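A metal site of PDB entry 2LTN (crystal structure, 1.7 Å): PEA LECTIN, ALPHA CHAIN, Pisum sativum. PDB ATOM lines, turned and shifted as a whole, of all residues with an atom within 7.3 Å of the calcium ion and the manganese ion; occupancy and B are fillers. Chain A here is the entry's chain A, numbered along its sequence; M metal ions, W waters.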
ATOM      1  N   ASP A  81       3.778 -24.162  17.862  1.00  0.00           N
ATOM      2  CA  ASP A  81       4.609 -24.468  16.796  1.00  0.00           C
ATOM      3  C   ASP A  81       5.382 -25.772  16.767  1.00  0.00           C
ATOM      4  O   ASP A  81       5.513 -26.554  15.780  1.00  0.00           O
ATOM      5  CB  ASP A  81       5.336 -23.388  15.981  1.00  0.00           C
ATOM      6  CG  ASP A  81       4.412 -22.652  15.044  1.00  0.00           C
ATOM      7  OD1 ASP A  81       3.913 -21.555  15.306  1.00  0.00           O
ATOM      8  OD2 ASP A  81       4.179 -23.153  13.878  1.00  0.00           O
ATOM      9  N   GLY A  82       6.089 -25.995  17.900  1.00  0.00           N
ATOM     10  CA  GLY A  82       6.872 -27.245  18.066  1.00  0.00           C
ATOM     11  C   GLY A  82       8.153 -26.878  18.943  1.00  0.00           C
ATOM     12  O   GLY A  82       8.113 -25.802  19.493  1.00  0.00           O
ATOM     13  N   GLY A  98       7.670 -18.721  15.451  1.00  0.00           N
ATOM     14  CA  GLY A  98       6.516 -19.443  14.756  1.00  0.00           C
ATOM     15  C   GLY A  98       7.018 -20.729  14.145  1.00  0.00           C
ATOM     16  O   GLY A  98       7.633 -21.514  14.804  1.00  0.00           O
ATOM     17  N   GLY A  99       6.625 -20.900  12.795  1.00  0.00           N
ATOM     18  CA  GLY A  99       7.026 -22.138  12.149  1.00  0.00           C
ATOM     19  C   GLY A  99       8.488 -22.471  11.980  1.00  0.00           C
ATOM     20  O   GLY A  99       8.890 -23.572  11.655  1.00  0.00           O
ATOM     21  N   TYR A 100       9.332 -21.404  12.222  1.00  0.00           N
ATOM     22  CA  TYR A 100      10.784 -21.513  12.122  1.00  0.00           C
ATOM     23  C   TYR A 100      11.463 -22.003  13.435  1.00  0.00           C
ATOM     24  O   TYR A 100      12.659 -22.305  13.409  1.00  0.00           O
ATOM     25  CB  TYR A 100      11.397 -20.196  11.643  1.00  0.00           C
ATOM     26  CG  TYR A 100      10.945 -19.855  10.203  1.00  0.00           C
ATOM     27  CD1 TYR A 100      11.603 -20.398   9.132  1.00  0.00           C
ATOM     28  CD2 TYR A 100       9.836 -19.046  10.045  1.00  0.00           C
ATOM     29  CE1 TYR A 100      11.198 -20.038   7.826  1.00  0.00           C
ATOM     30  CE2 TYR A 100       9.366 -18.752   8.744  1.00  0.00           C
ATOM     31  CZ  TYR A 100      10.112 -19.230   7.665  1.00  0.00           C
ATOM     32  OH  TYR A 100       9.675 -18.884   6.392  1.00  0.00           O
ATOM     33  N   LEU A 101      10.629 -22.170  14.419  1.00  0.00           N
ATOM     34  CA  LEU A 101      10.981 -22.820  15.687  1.00  0.00           C
ATOM     35  C   LEU A 101      12.088 -22.088  16.481  1.00  0.00           C
ATOM     36  O   LEU A 101      12.708 -22.779  17.345  1.00  0.00           O
ATOM     37  CB  LEU A 101      11.299 -24.346  15.467  1.00  0.00           C
ATOM     38  CG  LEU A 101      10.088 -25.111  14.759  1.00  0.00           C
ATOM     39  CD1 LEU A 101      10.493 -26.553  14.522  1.00  0.00           C
ATOM     40  CD2 LEU A 101       8.863 -24.918  15.580  1.00  0.00           C
ATOM     41  N   GLU A 119      13.598 -31.618  15.192  1.00  0.00           N
ATOM     42  CA  GLU A 119      12.347 -30.956  15.465  1.00  0.00           C
ATOM     43  C   GLU A 119      11.205 -31.860  15.799  1.00  0.00           C
ATOM     44  O   GLU A 119      11.216 -32.975  15.322  1.00  0.00           O
ATOM     45  CB  GLU A 119      11.948 -29.977  14.331  1.00  0.00           C
ATOM     46  CG  GLU A 119      11.686 -30.891  13.028  1.00  0.00           C
ATOM     47  CD  GLU A 119      11.054 -30.026  11.986  1.00  0.00           C
ATOM     48  OE1 GLU A 119       9.961 -30.398  11.457  1.00  0.00           O
ATOM     49  OE2 GLU A 119      11.552 -28.944  11.664  1.00  0.00           O
ATOM     50  N   PHE A 120      10.330 -31.466  16.637  1.00  0.00           N
ATOM     51  CA  PHE A 120       9.073 -32.145  17.066  1.00  0.00           C
ATOM     52  C   PHE A 120       8.062 -31.070  16.704  1.00  0.00           C
ATOM     53  O   PHE A 120       7.758 -30.103  17.394  1.00  0.00           O
ATOM     54  CB  PHE A 120       9.074 -32.542  18.563  1.00  0.00           C
ATOM     55  CG  PHE A 120      10.256 -33.382  18.906  1.00  0.00           C
ATOM     56  CD1 PHE A 120      11.512 -32.740  19.138  1.00  0.00           C
ATOM     57  CD2 PHE A 120      10.215 -34.778  18.927  1.00  0.00           C
ATOM     58  CE1 PHE A 120      12.625 -33.464  19.425  1.00  0.00           C
ATOM     59  CE2 PHE A 120      11.359 -35.541  19.225  1.00  0.00           C
ATOM     60  CZ  PHE A 120      12.565 -34.856  19.471  1.00  0.00           C
ATOM     61  N   ASP A 121       7.578 -31.256  15.432  1.00  0.00           N
ATOM     62  CA  ASP A 121       6.780 -30.192  14.762  1.00  0.00           C
ATOM     63  C   ASP A 121       5.279 -30.448  14.850  1.00  0.00           C
ATOM     64  O   ASP A 121       4.870 -31.534  14.440  1.00  0.00           O
ATOM     65  CB  ASP A 121       7.346 -30.136  13.311  1.00  0.00           C
ATOM     66  CG  ASP A 121       6.743 -29.015  12.513  1.00  0.00           C
ATOM     67  OD1 ASP A 121       5.736 -28.361  12.965  1.00  0.00           O
ATOM     68  OD2 ASP A 121       7.322 -28.731  11.460  1.00  0.00           O
ATOM     69  N   THR A 122       4.577 -29.562  15.475  1.00  0.00           N
ATOM     70  CA  THR A 122       3.151 -29.821  15.798  1.00  0.00           C
ATOM     71  C   THR A 122       2.206 -29.120  14.842  1.00  0.00           C
ATOM     72  O   THR A 122       0.994 -29.279  15.110  1.00  0.00           O
ATOM     73  CB  THR A 122       2.886 -29.471  17.322  1.00  0.00           C
ATOM     74  OG1 THR A 122       3.226 -28.033  17.424  1.00  0.00           O
ATOM     75  CG2 THR A 122       3.605 -30.369  18.303  1.00  0.00           C
ATOM     76  N   PHE A 123       2.752 -28.354  13.947  1.00  0.00           N
ATOM     77  CA  PHE A 123       1.808 -27.545  13.079  1.00  0.00           C
ATOM     78  C   PHE A 123       2.290 -27.631  11.665  1.00  0.00           C
ATOM     79  O   PHE A 123       3.437 -27.425  11.321  1.00  0.00           O
ATOM     80  CB  PHE A 123       1.686 -26.114  13.607  1.00  0.00           C
ATOM     81  CG  PHE A 123       0.963 -25.128  12.758  1.00  0.00           C
ATOM     82  CD1 PHE A 123       1.518 -24.367  11.776  1.00  0.00           C
ATOM     83  CD2 PHE A 123      -0.439 -24.971  13.083  1.00  0.00           C
ATOM     84  CE1 PHE A 123       0.794 -23.433  11.056  1.00  0.00           C
ATOM     85  CE2 PHE A 123      -1.200 -24.012  12.348  1.00  0.00           C
ATOM     86  CZ  PHE A 123      -0.569 -23.335  11.316  1.00  0.00           C
ATOM     87  N   TYR A 124       1.266 -27.886  10.735  1.00  0.00           N
ATOM     88  CA  TYR A 124       1.668 -28.006   9.305  1.00  0.00           C
ATOM     89  C   TYR A 124       1.778 -26.682   8.635  1.00  0.00           C
ATOM     90  O   TYR A 124       0.817 -25.875   8.588  1.00  0.00           O
ATOM     91  CB  TYR A 124       0.469 -28.832   8.651  1.00  0.00           C
ATOM     92  CG  TYR A 124       0.541 -28.779   7.134  1.00  0.00           C
ATOM     93  CD1 TYR A 124       1.550 -29.443   6.463  1.00  0.00           C
ATOM     94  CD2 TYR A 124      -0.436 -28.108   6.428  1.00  0.00           C
ATOM     95  CE1 TYR A 124       1.639 -29.410   5.070  1.00  0.00           C
ATOM     96  CE2 TYR A 124      -0.391 -28.082   5.004  1.00  0.00           C
ATOM     97  CZ  TYR A 124       0.620 -28.752   4.363  1.00  0.00           C
ATOM     98  OH  TYR A 124       0.670 -28.705   2.977  1.00  0.00           O
ATOM     99  N   ASN A 125       2.978 -26.427   8.153  1.00  0.00           N
ATOM    100  CA  ASN A 125       3.320 -25.212   7.385  1.00  0.00           C
ATOM    101  C   ASN A 125       3.357 -25.707   5.898  1.00  0.00           C
ATOM    102  O   ASN A 125       4.273 -26.393   5.534  1.00  0.00           O
ATOM    103  CB  ASN A 125       4.705 -24.620   7.784  1.00  0.00           C
ATOM    104  CG  ASN A 125       4.614 -24.104   9.230  1.00  0.00           C
ATOM    105  OD1 ASN A 125       4.902 -24.814  10.193  1.00  0.00           O
ATOM    106  ND2 ASN A 125       4.123 -22.878   9.355  1.00  0.00           N
ATOM    107  N   ALA A 126       2.281 -25.252   5.200  1.00  0.00           N
ATOM    108  CA  ALA A 126       2.235 -25.712   3.757  1.00  0.00           C
ATOM    109  C   ALA A 126       3.429 -25.458   2.932  1.00  0.00           C
ATOM    110  O   ALA A 126       3.769 -26.311   1.995  1.00  0.00           O
ATOM    111  CB  ALA A 126       0.967 -25.047   3.152  1.00  0.00           C
ATOM    112  N   TRP A 128       6.570 -25.887   3.400  1.00  0.00           N
ATOM    113  CA  TRP A 128       7.626 -26.851   3.551  1.00  0.00           C
ATOM    114  C   TRP A 128       7.382 -28.090   4.355  1.00  0.00           C
ATOM    115  O   TRP A 128       8.305 -28.955   4.161  1.00  0.00           O
ATOM    116  CB  TRP A 128       8.903 -26.056   4.150  1.00  0.00           C
ATOM    117  CG  TRP A 128       8.586 -25.587   5.560  1.00  0.00           C
ATOM    118  CD1 TRP A 128       8.592 -26.322   6.711  1.00  0.00           C
ATOM    119  CD2 TRP A 128       8.351 -24.226   5.951  1.00  0.00           C
ATOM    120  NE1 TRP A 128       8.201 -25.541   7.744  1.00  0.00           N
ATOM    121  CE2 TRP A 128       8.082 -24.262   7.345  1.00  0.00           C
ATOM    122  CE3 TRP A 128       8.266 -23.031   5.243  1.00  0.00           C
ATOM    123  CZ2 TRP A 128       7.782 -23.105   8.086  1.00  0.00           C
ATOM    124  CZ3 TRP A 128       7.978 -21.892   5.972  1.00  0.00           C
ATOM    125  CH2 TRP A 128       7.700 -21.926   7.371  1.00  0.00           C
ATOM    126  N   ASP A 129       6.356 -28.271   5.161  1.00  0.00           N
ATOM    127  CA  ASP A 129       6.196 -29.509   5.944  1.00  0.00           C
ATOM    128  C   ASP A 129       5.634 -30.645   5.028  1.00  0.00           C
ATOM    129  O   ASP A 129       5.040 -30.237   3.990  1.00  0.00           O
ATOM    130  CB  ASP A 129       5.268 -29.247   7.136  1.00  0.00           C
ATOM    131  CG  ASP A 129       6.047 -28.546   8.351  1.00  0.00           C
ATOM    132  OD1 ASP A 129       7.249 -28.887   8.357  1.00  0.00           O
ATOM    133  OD2 ASP A 129       5.310 -27.889   9.040  1.00  0.00           O
ATOM    134  N   PRO A 130       5.701 -31.829   5.493  1.00  0.00           N
ATOM    135  CA  PRO A 130       5.166 -33.006   4.748  1.00  0.00           C
ATOM    136  C   PRO A 130       3.679 -32.752   4.399  1.00  0.00           C
ATOM    137  O   PRO A 130       2.860 -32.412   5.241  1.00  0.00           O
ATOM    138  CB  PRO A 130       5.379 -34.154   5.693  1.00  0.00           C
ATOM    139  CG  PRO A 130       6.631 -33.774   6.513  1.00  0.00           C
ATOM    140  CD  PRO A 130       6.451 -32.258   6.730  1.00  0.00           C
ATOM    141  N   ASP A 134       0.656 -34.435   8.767  1.00  0.00           N
ATOM    142  CA  ASP A 134       0.844 -35.084  10.061  1.00  0.00           C
ATOM    143  C   ASP A 134       1.899 -34.257  10.922  1.00  0.00           C
ATOM    144  O   ASP A 134       2.786 -33.736  10.271  1.00  0.00           O
ATOM    145  CB  ASP A 134       1.465 -36.467   9.999  1.00  0.00           C
ATOM    146  CG  ASP A 134       0.481 -37.511   9.420  1.00  0.00           C
ATOM    147  OD1 ASP A 134      -0.724 -37.164   9.385  1.00  0.00           O
ATOM    148  OD2 ASP A 134       1.074 -38.574   9.094  1.00  0.00           O
ATOM    149  N   HIS A 136       5.161 -34.326  13.099  1.00  0.00           N
ATOM    150  CA  HIS A 136       6.282 -35.141  12.724  1.00  0.00           C
ATOM    151  C   HIS A 136       7.604 -34.788  13.494  1.00  0.00           C
ATOM    152  O   HIS A 136       7.598 -33.651  14.009  1.00  0.00           O
ATOM    153  CB  HIS A 136       6.589 -34.901  11.182  1.00  0.00           C
ATOM    154  CG  HIS A 136       6.614 -33.460  10.758  1.00  0.00           C
ATOM    155  ND1 HIS A 136       5.476 -32.737  10.492  1.00  0.00           N
ATOM    156  CD2 HIS A 136       7.665 -32.615  10.527  1.00  0.00           C
ATOM    157  CE1 HIS A 136       5.829 -31.472  10.172  1.00  0.00           C
ATOM    158  NE2 HIS A 136       7.129 -31.411  10.172  1.00  0.00           N
ATOM    159  N   ILE A 137       8.434 -35.748  13.440  1.00  0.00           N
ATOM    160  CA  ILE A 137       9.818 -35.511  13.966  1.00  0.00           C
ATOM    161  C   ILE A 137      10.603 -35.261  12.706  1.00  0.00           C
ATOM    162  O   ILE A 137      10.383 -36.007  11.674  1.00  0.00           O
ATOM    163  CB  ILE A 137      10.310 -36.805  14.686  1.00  0.00           C
ATOM    164  CG1 ILE A 137       9.411 -37.009  15.951  1.00  0.00           C
ATOM    165  CG2 ILE A 137      11.824 -36.703  15.013  1.00  0.00           C
ATOM    166  CD1 ILE A 137       9.418 -38.542  16.334  1.00  0.00           C
ATOM    167  N   GLY A 138      11.611 -34.393  12.676  1.00  0.00           N
ATOM    168  CA  GLY A 138      12.434 -34.084  11.616  1.00  0.00           C
ATOM    169  C   GLY A 138      13.910 -33.744  11.956  1.00  0.00           C
ATOM    170  O   GLY A 138      14.088 -33.285  13.092  1.00  0.00           O
ATOM    171  N   ASP A 140      16.748 -31.373  10.784  1.00  0.00           N
ATOM    172  CA  ASP A 140      16.906 -30.127  10.096  1.00  0.00           C
ATOM    173  C   ASP A 140      18.391 -29.741  10.013  1.00  0.00           C
ATOM    174  O   ASP A 140      19.068 -29.730  11.073  1.00  0.00           O
ATOM    175  CB  ASP A 140      16.146 -28.965  10.741  1.00  0.00           C
ATOM    176  CG  ASP A 140      14.685 -29.146  10.879  1.00  0.00           C
ATOM    177  OD1 ASP A 140      14.196 -30.136  10.237  1.00  0.00           O
ATOM    178  OD2 ASP A 140      13.951 -28.469  11.623  1.00  0.00           O
ATOM    179  N   ILE A 144      14.590 -24.993   7.630  1.00  0.00           N
ATOM    180  CA  ILE A 144      13.392 -25.518   8.325  1.00  0.00           C
ATOM    181  C   ILE A 144      12.699 -26.708   7.541  1.00  0.00           C
ATOM    182  O   ILE A 144      11.819 -27.358   8.067  1.00  0.00           O
ATOM    183  CB  ILE A 144      12.388 -24.403   8.615  1.00  0.00           C
ATOM    184  CG1 ILE A 144      11.379 -24.728   9.673  1.00  0.00           C
ATOM    185  CG2 ILE A 144      11.715 -23.811   7.321  1.00  0.00           C
ATOM    186  CD1 ILE A 144      11.984 -25.087  11.076  1.00  0.00           C
ATOM    187  N   LYS A 145      13.180 -26.838   6.334  1.00  0.00           N
ATOM    188  CA  LYS A 145      12.687 -27.948   5.461  1.00  0.00           C
ATOM    189  C   LYS A 145      13.537 -29.172   5.769  1.00  0.00           C
ATOM    190  O   LYS A 145      14.709 -29.178   5.296  1.00  0.00           O
ATOM    191  CB  LYS A 145      12.750 -27.590   3.952  1.00  0.00           C
ATOM    192  CG  LYS A 145      12.044 -28.825   3.232  1.00  0.00           C
ATOM    193  CD  LYS A 145      11.848 -28.530   1.763  1.00  0.00           C
ATOM    194  CE  LYS A 145      12.996 -28.825   0.866  1.00  0.00           C
ATOM    195  NZ  LYS A 145      13.408 -30.260   0.842  1.00  0.00           N
ATOM    196  N   SER A 146      13.001 -30.073   6.570  1.00  0.00           N
ATOM    197  CA  SER A 146      13.759 -31.232   7.035  1.00  0.00           C
ATOM    198  C   SER A 146      14.388 -32.108   5.989  1.00  0.00           C
ATOM    199  O   SER A 146      13.749 -32.276   4.853  1.00  0.00           O
ATOM    200  CB  SER A 146      12.874 -32.121   7.929  1.00  0.00           C
ATOM    201  OG  SER A 146      12.230 -31.328   8.911  1.00  0.00           O
ATOM    202  N   THR A 149      11.875 -36.956   7.776  1.00  0.00           N
ATOM    203  CA  THR A 149      10.773 -36.767   8.727  1.00  0.00           C
ATOM    204  C   THR A 149      10.125 -38.123   8.979  1.00  0.00           C
ATOM    205  O   THR A 149      10.248 -39.051   8.140  1.00  0.00           O
ATOM    206  CB  THR A 149       9.701 -35.721   8.276  1.00  0.00           C
ATOM    207  OG1 THR A 149       9.188 -36.267   6.961  1.00  0.00           O
ATOM    208  CG2 THR A 149      10.202 -34.308   8.089  1.00  0.00           C
HETATM  209 CA    CA M   1       5.617 -26.709  11.125  1.00  0.00          CA
HETATM  210 MN    MN M   2       8.480 -29.638   9.999  1.00  0.00          MN
HETATM  211  O   HOH W   1       9.831 -27.837   9.936  1.00  0.00           O
HETATM  212  O   HOH W   2       5.519 -25.411  13.130  1.00  0.00           O
HETATM  213  O   HOH W   3       9.710 -30.561   8.508  1.00  0.00           O
HETATM  214  O   HOH W   4       7.798 -25.906  10.821  1.00  0.00           O
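The calcium ion is bound by the side-chain amide oxygen (OD1) of Asn 125, the backbone carbonyl oxygen (O) of Phe 123, water W4, water W2, the side-chain carboxylate (OD2) of Asp 129, the side-chain carboxylate (OD1) of Asp 121 and the side-chain carboxylate (OD2) of Asp 121.
The calcium ion has seven donor atoms within binding distance.
The manganese ion is bound by OD2 of Asp 121, 2.1 Å away.
Water W3 binds the manganese ion, at 2.1 Å.
OD1 of Asp 129 binds the manganese ion (2.2 Å).
OE1 of Glu 119 is bound to the manganese ion.
The manganese ion is bound by NE2 of His 136.
Water W1 is bound to the manganese ion, at 2.3 Å.
The manganese ion has six donor atoms within binding distance.
Of the 26 residues printed, 4 come within 4 Å of the manganese ion.
OE2 of Glu 119 lies close to OD2 of Asp 140, 2.4 Å away.
The backbone carbonyl oxygen (O) of Gly 138 is in hydrogen-bond range of the backbone NH (N) of Glu 119.
O of Asp 134 lies within hydrogen-bond range of ND1 of His 136 (2.9 Å).
Within 4 Å of the calcium ion: Asp 121, Phe 123, Asn 125 and Asp 129.
Water W4 bridges the backbone carbonyl oxygen (O) of Gly 99 and the indole nitrogen (NE1) of Trp 128.
Water W1 lies within hydrogen-bond range of the side-chain carboxylate of Glu 119 (2.7 Å) and the backbone carbonyl oxygen of Ile 144 (2.8 Å).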
